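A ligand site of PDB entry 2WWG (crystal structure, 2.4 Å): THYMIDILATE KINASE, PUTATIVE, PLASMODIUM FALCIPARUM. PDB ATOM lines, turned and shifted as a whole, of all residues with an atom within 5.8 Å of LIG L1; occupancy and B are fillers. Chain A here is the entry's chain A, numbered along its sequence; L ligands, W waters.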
ATOM      1  N   LEU A  18       3.655  11.987   6.105  1.00  0.00           N
ATOM      2  CA  LEU A  18       5.001  12.490   6.206  1.00  0.00           C
ATOM      3  C   LEU A  18       4.927  13.987   6.212  1.00  0.00           C
ATOM      4  O   LEU A  18       3.858  14.579   5.986  1.00  0.00           O
ATOM      5  CB  LEU A  18       5.864  12.042   5.014  1.00  0.00           C
ATOM      6  CG  LEU A  18       6.126  10.537   4.883  1.00  0.00           C
ATOM      7  CD1 LEU A  18       7.025  10.265   3.648  1.00  0.00           C
ATOM      8  CD2 LEU A  18       6.803   9.970   6.129  1.00  0.00           C
ATOM      9  N   ASP A  19       6.097  14.610   6.445  1.00  0.00           N
ATOM     10  CA  ASP A  19       6.191  16.055   6.496  1.00  0.00           C
ATOM     11  C   ASP A  19       5.990  16.694   5.105  1.00  0.00           C
ATOM     12  O   ASP A  19       6.579  16.238   4.085  1.00  0.00           O
ATOM     13  CB  ASP A  19       7.542  16.433   7.084  1.00  0.00           C
ATOM     14  CG  ASP A  19       7.667  15.961   8.546  1.00  0.00           C
ATOM     15  OD1 ASP A  19       7.261  16.748   9.399  1.00  0.00           O
ATOM     16  OD2 ASP A  19       8.096  14.821   8.857  1.00  0.00           O
ATOM     17  N   ARG A  20       5.168  17.759   5.120  1.00  0.00           N
ATOM     18  CA  ARG A  20       4.808  18.538   3.946  1.00  0.00           C
ATOM     19  C   ARG A  20       4.030  17.687   2.916  1.00  0.00           C
ATOM     20  O   ARG A  20       4.236  17.823   1.705  1.00  0.00           O
ATOM     21  CB  ARG A  20       6.057  19.134   3.264  1.00  0.00           C
ATOM     22  CG  ARG A  20       6.972  20.052   4.061  1.00  0.00           C
ATOM     23  CD  ARG A  20       6.257  20.969   4.971  1.00  0.00           C
ATOM     24  NE  ARG A  20       6.953  22.252   5.095  1.00  0.00           N
ATOM     25  CZ  ARG A  20       7.701  22.637   6.126  1.00  0.00           C
ATOM     26  NH1 ARG A  20       7.903  21.848   7.162  1.00  0.00           N
ATOM     27  NH2 ARG A  20       8.235  23.824   6.099  1.00  0.00           N
ATOM     28  N   SER A  21       3.222  16.760   3.389  1.00  0.00           N
ATOM     29  CA  SER A  21       2.440  15.949   2.508  1.00  0.00           C
ATOM     30  C   SER A  21       1.044  16.526   2.154  1.00  0.00           C
ATOM     31  O   SER A  21       0.335  15.925   1.409  1.00  0.00           O
ATOM     32  CB  SER A  21       2.400  14.512   3.011  1.00  0.00           C
ATOM     33  OG  SER A  21       1.692  14.389   4.225  1.00  0.00           O
ATOM     34  N   GLY A  22       0.682  17.731   2.654  1.00  0.00           N
ATOM     35  CA  GLY A  22      -0.618  18.360   2.368  1.00  0.00           C
ATOM     36  C   GLY A  22      -1.701  18.135   3.443  1.00  0.00           C
ATOM     37  O   GLY A  22      -2.908  18.366   3.161  1.00  0.00           O
ATOM     38  N   LYS A  23      -1.310  17.669   4.639  1.00  0.00           N
ATOM     39  CA  LYS A  23      -2.261  17.497   5.801  1.00  0.00           C
ATOM     40  C   LYS A  23      -3.036  18.759   6.070  1.00  0.00           C
ATOM     41  O   LYS A  23      -4.279  18.743   6.107  1.00  0.00           O
ATOM     42  CB  LYS A  23      -1.514  17.041   7.073  1.00  0.00           C
ATOM     43  CG  LYS A  23      -1.016  15.589   6.930  1.00  0.00           C
ATOM     44  CD  LYS A  23      -0.398  15.022   8.158  1.00  0.00           C
ATOM     45  CE  LYS A  23       1.083  15.265   8.264  1.00  0.00           C
ATOM     46  NZ  LYS A  23       1.624  16.594   8.018  1.00  0.00           N
ATOM     47  N   SER A  24      -2.317  19.851   6.221  1.00  0.00           N
ATOM     48  CA  SER A  24      -2.966  21.116   6.506  1.00  0.00           C
ATOM     49  C   SER A  24      -3.882  21.581   5.395  1.00  0.00           C
ATOM     50  O   SER A  24      -4.952  22.134   5.666  1.00  0.00           O
ATOM     51  CB  SER A  24      -1.935  22.216   6.759  1.00  0.00           C
ATOM     52  OG  SER A  24      -1.437  22.019   8.068  1.00  0.00           O
ATOM     53  N   THR A  25      -3.411  21.412   4.166  1.00  0.00           N
ATOM     54  CA  THR A  25      -4.178  21.768   3.002  1.00  0.00           C
ATOM     55  C   THR A  25      -5.477  20.980   2.949  1.00  0.00           C
ATOM     56  O   THR A  25      -6.560  21.566   2.813  1.00  0.00           O
ATOM     57  CB  THR A  25      -3.354  21.524   1.720  1.00  0.00           C
ATOM     58  OG1 THR A  25      -2.130  22.263   1.796  1.00  0.00           O
ATOM     59  CG2 THR A  25      -4.148  21.993   0.522  1.00  0.00           C
ATOM     60  N   GLN A  26      -5.365  19.665   3.069  1.00  0.00           N
ATOM     61  CA  GLN A  26      -6.523  18.802   3.004  1.00  0.00           C
ATOM     62  C   GLN A  26      -7.435  18.994   4.198  1.00  0.00           C
ATOM     63  O   GLN A  26      -8.673  18.986   4.026  1.00  0.00           O
ATOM     64  CB  GLN A  26      -6.107  17.323   2.829  1.00  0.00           C
ATOM     65  CG  GLN A  26      -5.435  17.042   1.434  1.00  0.00           C
ATOM     66  CD  GLN A  26      -6.345  17.551   0.250  1.00  0.00           C
ATOM     67  OE1 GLN A  26      -7.563  17.450   0.312  1.00  0.00           O
ATOM     68  NE2 GLN A  26      -5.746  18.184  -0.745  1.00  0.00           N
ATOM     69  N   ASP A 100      -4.963  17.461  12.238  1.00  0.00           N
ATOM     70  CA  ASP A 100      -3.682  17.036  11.631  1.00  0.00           C
ATOM     71  C   ASP A 100      -2.850  16.376  12.699  1.00  0.00           C
ATOM     72  O   ASP A 100      -2.496  16.987  13.724  1.00  0.00           O
ATOM     73  CB  ASP A 100      -2.832  18.186  11.096  1.00  0.00           C
ATOM     74  CG  ASP A 100      -3.596  19.088  10.168  1.00  0.00           C
ATOM     75  OD1 ASP A 100      -4.524  18.532   9.565  1.00  0.00           O
ATOM     76  OD2 ASP A 100      -3.273  20.327  10.036  1.00  0.00           O
ATOM     77  N   ARG A 101      -2.566  15.121  12.460  1.00  0.00           N
ATOM     78  CA  ARG A 101      -1.704  14.323  13.310  1.00  0.00           C
ATOM     79  C   ARG A 101      -2.413  13.850  14.545  1.00  0.00           C
ATOM     80  O   ARG A 101      -3.218  14.582  15.121  1.00  0.00           O
ATOM     81  CB  ARG A 101      -0.371  15.017  13.618  1.00  0.00           C
ATOM     82  CG  ARG A 101       0.454  15.281  12.382  1.00  0.00           C
ATOM     83  CD  ARG A 101       1.951  15.345  12.772  1.00  0.00           C
ATOM     84  NE  ARG A 101       2.833  15.702  11.671  1.00  0.00           N
ATOM     85  CZ  ARG A 101       3.365  14.845  10.817  1.00  0.00           C
ATOM     86  NH1 ARG A 101       3.132  13.520  10.918  1.00  0.00           N
ATOM     87  NH2 ARG A 101       4.140  15.304   9.861  1.00  0.00           N
ATOM     88  N   TYR A 143       9.386  12.471  -2.077  1.00  0.00           N
ATOM     89  CA  TYR A 143       8.465  13.264  -2.858  1.00  0.00           C
ATOM     90  C   TYR A 143       8.374  14.783  -2.479  1.00  0.00           C
ATOM     91  O   TYR A 143       8.356  15.648  -3.349  1.00  0.00           O
ATOM     92  CB  TYR A 143       7.107  12.574  -2.898  1.00  0.00           C
ATOM     93  CG  TYR A 143       6.051  13.403  -3.563  1.00  0.00           C
ATOM     94  CD1 TYR A 143       6.008  13.540  -4.952  1.00  0.00           C
ATOM     95  CD2 TYR A 143       5.085  14.052  -2.787  1.00  0.00           C
ATOM     96  CE1 TYR A 143       5.041  14.295  -5.550  1.00  0.00           C
ATOM     97  CE2 TYR A 143       4.105  14.813  -3.377  1.00  0.00           C
ATOM     98  CZ  TYR A 143       4.095  14.929  -4.749  1.00  0.00           C
ATOM     99  OH  TYR A 143       3.142  15.709  -5.313  1.00  0.00           O
ATOM    100  N   ARG A 147       8.794  21.155  -1.602  1.00  0.00           N
ATOM    101  CA  ARG A 147       7.706  22.045  -1.193  1.00  0.00           C
ATOM    102  C   ARG A 147       8.160  23.122  -0.209  1.00  0.00           C
ATOM    103  O   ARG A 147       9.024  22.851   0.634  1.00  0.00           O
ATOM    104  CB  ARG A 147       6.556  21.229  -0.590  1.00  0.00           C
ATOM    105  CG  ARG A 147       6.426  19.822  -1.157  1.00  0.00           C
ATOM    106  CD  ARG A 147       5.185  19.680  -2.007  1.00  0.00           C
ATOM    107  NE  ARG A 147       4.113  18.963  -1.318  1.00  0.00           N
ATOM    108  CZ  ARG A 147       3.175  18.258  -1.925  1.00  0.00           C
ATOM    109  NH1 ARG A 147       2.241  17.646  -1.217  1.00  0.00           N
ATOM    110  NH2 ARG A 147       3.166  18.172  -3.250  1.00  0.00           N
ATOM    111  N   SER A 148       7.591  24.315  -0.294  1.00  0.00           N
ATOM    112  CA  SER A 148       7.936  25.388   0.657  1.00  0.00           C
ATOM    113  C   SER A 148       8.657  24.954   1.953  1.00  0.00           C
ATOM    114  O   SER A 148       8.163  24.096   2.678  1.00  0.00           O
ATOM    115  CB  SER A 148       6.669  26.119   1.121  1.00  0.00           C
ATOM    116  OG  SER A 148       6.309  27.216   0.313  1.00  0.00           O
ATOM    117  N   ALA A 182      -1.349  10.879  -2.283  1.00  0.00           N
ATOM    118  CA  ALA A 182      -1.248  12.332  -2.186  1.00  0.00           C
ATOM    119  C   ALA A 182      -0.244  12.896  -3.166  1.00  0.00           C
ATOM    120  O   ALA A 182       0.185  14.039  -3.058  1.00  0.00           O
ATOM    121  CB  ALA A 182      -1.039  12.818  -0.713  1.00  0.00           C
ATOM    122  N   ARG A 184      -1.148  13.668  -6.110  1.00  0.00           N
ATOM    123  CA  ARG A 184      -2.031  14.241  -7.128  1.00  0.00           C
ATOM    124  C   ARG A 184      -2.359  15.686  -6.915  1.00  0.00           C
ATOM    125  O   ARG A 184      -1.781  16.336  -6.056  1.00  0.00           O
ATOM    126  CB  ARG A 184      -3.258  13.382  -7.238  1.00  0.00           C
ATOM    127  CG  ARG A 184      -2.822  12.009  -7.748  1.00  0.00           C
ATOM    128  CD  ARG A 184      -3.886  11.010  -7.741  1.00  0.00           C
ATOM    129  NE  ARG A 184      -4.311  10.714  -6.395  1.00  0.00           N
ATOM    130  CZ  ARG A 184      -5.557  10.759  -5.969  1.00  0.00           C
ATOM    131  NH1 ARG A 184      -6.517  11.064  -6.829  1.00  0.00           N
ATOM    132  NH2 ARG A 184      -5.838  10.476  -4.705  1.00  0.00           N
ATOM    133  N   LYS A 185      -3.264  16.218  -7.727  1.00  0.00           N
ATOM    134  CA  LYS A 185      -3.706  17.594  -7.574  1.00  0.00           C
ATOM    135  C   LYS A 185      -4.496  17.673  -6.309  1.00  0.00           C
ATOM    136  O   LYS A 185      -5.251  16.747  -5.974  1.00  0.00           O
ATOM    137  CB  LYS A 185      -4.592  18.020  -8.757  1.00  0.00           C
ATOM    138  CG  LYS A 185      -3.801  18.414  -9.997  1.00  0.00           C
ATOM    139  CD  LYS A 185      -4.654  18.538 -11.278  1.00  0.00           C
ATOM    140  CE  LYS A 185      -4.588  17.238 -12.125  1.00  0.00           C
ATOM    141  NZ  LYS A 185      -5.935  16.900 -12.701  1.00  0.00           N
ATOM    142  N   ILE A 186      -4.338  18.807  -5.635  1.00  0.00           N
ATOM    143  CA  ILE A 186      -5.105  19.160  -4.437  1.00  0.00           C
ATOM    144  C   ILE A 186      -6.589  18.768  -4.569  1.00  0.00           C
ATOM    145  O   ILE A 186      -7.142  18.086  -3.668  1.00  0.00           O
ATOM    146  CB  ILE A 186      -4.909  20.654  -4.077  1.00  0.00           C
ATOM    147  CG1 ILE A 186      -3.533  20.920  -3.478  1.00  0.00           C
ATOM    148  CG2 ILE A 186      -5.932  21.095  -3.048  1.00  0.00           C
ATOM    149  CD1 ILE A 186      -3.080  22.468  -3.564  1.00  0.00           C
ATOM    150  N   ILE A 189      -7.170  14.902  -4.571  1.00  0.00           N
ATOM    151  CA  ILE A 189      -7.045  14.391  -3.220  1.00  0.00           C
ATOM    152  C   ILE A 189      -8.316  14.778  -2.490  1.00  0.00           C
ATOM    153  O   ILE A 189      -8.963  13.938  -1.871  1.00  0.00           O
ATOM    154  CB  ILE A 189      -5.738  14.881  -2.448  1.00  0.00           C
ATOM    155  CG1 ILE A 189      -4.457  14.454  -3.171  1.00  0.00           C
ATOM    156  CG2 ILE A 189      -5.664  14.208  -1.118  1.00  0.00           C
ATOM    157  CD1 ILE A 189      -3.240  15.373  -2.967  1.00  0.00           C
HETATM  158  P1  LIG L   1       1.607  19.448   5.870  1.00  0.00           P
HETATM  159  O1  LIG L   1       2.881  19.975   6.520  1.00  0.00           O
HETATM  160  O2  LIG L   1       0.495  19.911   6.803  1.00  0.00           O
HETATM  161  O3  LIG L   1       1.690  18.017   5.793  1.00  0.00           O
HETATM  162  P2  LIG L   1       0.878  21.446   3.955  1.00  0.00           P
HETATM  163  O4  LIG L   1       1.341  22.648   4.903  1.00  0.00           O
HETATM  164  O5  LIG L   1      -0.629  21.335   3.939  1.00  0.00           O
HETATM  165  O6  LIG L   1       1.551  20.089   4.416  1.00  0.00           O
HETATM  166  O7  LIG L   1       1.568  21.671   2.589  1.00  0.00           O
HETATM  167  C1  LIG L   1       2.957  21.604   2.376  1.00  0.00           C
HETATM  168  C2  LIG L   1       3.304  22.541   1.164  1.00  0.00           C
HETATM  169  O8  LIG L   1       3.009  21.935  -0.184  1.00  0.00           O
HETATM  170  C3  LIG L   1       2.451  23.830   1.193  1.00  0.00           C
HETATM  171  O9  LIG L   1       3.118  24.867   0.497  1.00  0.00           O
HETATM  172  C4  LIG L   1       1.212  23.406   0.369  1.00  0.00           C
HETATM  173  O10 LIG L   1       0.693  24.529  -0.265  1.00  0.00           O
HETATM  174  C5  LIG L   1       1.815  22.570  -0.716  1.00  0.00           C
HETATM  175  N1  LIG L   1       0.935  21.491  -1.184  1.00  0.00           N
HETATM  176  C6  LIG L   1       0.117  20.713  -0.451  1.00  0.00           C
HETATM  177  N2  LIG L   1      -0.494  19.854  -1.234  1.00  0.00           N
HETATM  178  C7  LIG L   1      -0.053  20.063  -2.472  1.00  0.00           C
HETATM  179  C8  LIG L   1      -0.352  19.462  -3.691  1.00  0.00           C
HETATM  180  N3  LIG L   1      -1.228  18.413  -3.719  1.00  0.00           N
HETATM  181  N4  LIG L   1       0.281  19.945  -4.807  1.00  0.00           N
HETATM  182  C9  LIG L   1       1.113  20.973  -4.763  1.00  0.00           C
HETATM  183  N5  LIG L   1       1.409  21.571  -3.597  1.00  0.00           N
HETATM  184  C10 LIG L   1       0.835  21.105  -2.453  1.00  0.00           C
HETATM  185  P1  LG2 L   2       4.074  19.419  11.861  1.00  0.00           P
HETATM  186  O1  LG2 L   2       2.850  20.205  12.507  1.00  0.00           O
HETATM  187  O2  LG2 L   2       3.359  18.169  11.289  1.00  0.00           O
HETATM  188  O3  LG2 L   2       4.728  20.247  10.870  1.00  0.00           O
HETATM  189  O4  LG2 L   2       4.825  18.730  13.214  1.00  0.00           O
HETATM  190  C1  LG2 L   2       6.110  18.758  13.333  1.00  0.00           C
HETATM  191  C2  LG2 L   2       6.677  17.378  13.598  1.00  0.00           C
HETATM  192  O5  LG2 L   2       6.311  16.776  14.832  1.00  0.00           O
HETATM  193  C3  LG2 L   2       6.416  16.328  12.527  1.00  0.00           C
HETATM  194  O6  LG2 L   2       7.761  16.149  12.072  1.00  0.00           O
HETATM  195  C4  LG2 L   2       5.992  15.084  13.238  1.00  0.00           C
HETATM  196  C5  LG2 L   2       6.609  15.368  14.637  1.00  0.00           C
HETATM  197  N1  LG2 L   2       5.804  14.631  15.592  1.00  0.00           N
HETATM  198  C6  LG2 L   2       4.467  14.754  15.789  1.00  0.00           C
HETATM  199  N2  LG2 L   2       4.098  13.869  16.715  1.00  0.00           N
HETATM  200  C7  LG2 L   2       5.181  13.202  17.146  1.00  0.00           C
HETATM  201  C8  LG2 L   2       5.366  12.205  18.101  1.00  0.00           C
HETATM  202  O7  LG2 L   2       4.428  11.779  18.789  1.00  0.00           O
HETATM  203  N3  LG2 L   2       6.619  11.685  18.262  1.00  0.00           N
HETATM  204  C9  LG2 L   2       7.706  12.199  17.524  1.00  0.00           C
HETATM  205  N4  LG2 L   2       8.951  11.704  17.721  1.00  0.00           N
HETATM  206  N5  LG2 L   2       7.501  13.190  16.619  1.00  0.00           N
HETATM  207  C10 LG2 L   2       6.274  13.680  16.429  1.00  0.00           C
HETATM  208  O   HOH W   1       3.937  22.389   5.948  1.00  0.00           O
HETATM  209  O   HOH W   2       2.646  21.409   9.162  1.00  0.00           O
HETATM  210  O   HOH W   3      -0.004  24.699   4.240  1.00  0.00           O
HETATM  211  O   HOH W   4       3.735  18.208   8.102  1.00  0.00           O
HETATM  212  O   HOH W   5       0.949  18.437   9.876  1.00  0.00           O
HETATM  213  O   HOH W   6       0.969  23.033   7.416  1.00  0.00           O
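The side-chain amino group of Lys 23 lies within salt-bridge range of an oxygen (O3) of LIG L1.
N of Ser 21 lies within hydrogen-bond range of O3 of LIG L1 (3.1 Å).
NE of Arg 147 lies within hydrogen-bond range of O8 of LIG L1, 3.4 Å away.
The backbone NH of Ser 24 is in hydrogen-bond range of an oxygen (O2) of LIG L1.
OG1 of Thr 25 is in hydrogen-bond range of O5 of LIG L1 (2.8 Å).
O2 of LG2 L2 is in salt-bridge range of NE of Arg 101, at 2.6 Å.
An oxygen (O5) of LIG L1 sits at hydrogen-bond distance from the backbone NH (N) of Thr 25 (2.8 Å).
The backbone carbonyl oxygen (O) of Arg 184 is in hydrogen-bond range of a nitrogen (N3) of LIG L1 (3.2 Å).
The backbone NH (N) of Gly 22 is in hydrogen-bond range of an oxygen (O6) of LIG L1, 3.1 Å away.
The side-chain hydroxyl (OG) of Ser 24 sits at hydrogen-bond distance from an oxygen (O2) of LIG L1, 3.1 Å away.
N of Lys 23 is in hydrogen-bond range of O3 of LIG L1, 3.2 Å away.
O1 of LIG L1 lies within hydrogen-bond range of N of Arg 20.
OD1 of Asp 19 sits at hydrogen-bond distance from O6 of LG2 L2, 2.8 Å away.
NE of Arg 20 sits at hydrogen-bond distance from O of Ser 148 (3.3 Å).
The backbone carbonyl oxygen of Arg 20 is in hydrogen-bond range of the guanidinium group of Arg 147, at 3.2 Å.
The backbone carbonyl oxygen of Ile 186 lies within hydrogen-bond range of the side-chain amide nitrogen of Gln 26 (3.2 Å).
The side-chain hydroxyl of Ser 24 is in hydrogen-bond range of the side-chain carboxylate of Asp 100.
The guanidinium group (NH2) of Arg 147 lies within hydrogen-bond range of the side-chain hydroxyl (OH) of Tyr 143.
The side-chain hydroxyl of Ser 21 lies within hydrogen-bond range of the backbone carbonyl oxygen of Leu 18 (2.8 Å).
Ser 148 touches LIG L1 (CB to O9, 3.8 Å).
CG1 of Ile 186 touches N3 of LIG L1, at 3.4 Å.
Ile 189 touches LIG L1 (CD1 to N3, 3.7 Å).
11 residues have an atom within 4 Å of LIG L1: Arg 20, Ser 21, Gly 22, Lys 23, Ser 24, Thr 25, Arg 147, Ser 148, Arg 184, Ile 186 and Ile 189.
The nearest printed residue that does not touch LIG L1 is Leu 18 (4.1 Å).
Water W6 bridges O4 of LIG L1 (2.6 Å) and OG of Ser 24 (2.7 Å).
Water W1 bridges O1 of LIG L1 (2.7 Å) and NE of Arg 20 (3.1 Å).
Water W2 lies within hydrogen-bond range of an oxygen (O3) of LG2 L2 and an oxygen (O1) of LIG L1.
Water W5 lies within hydrogen-bond range of NZ of Lys 23 (2.7 Å), O2 of LG2 L2 (2.8 Å) and O2 of LIG L1 (3.4 Å).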
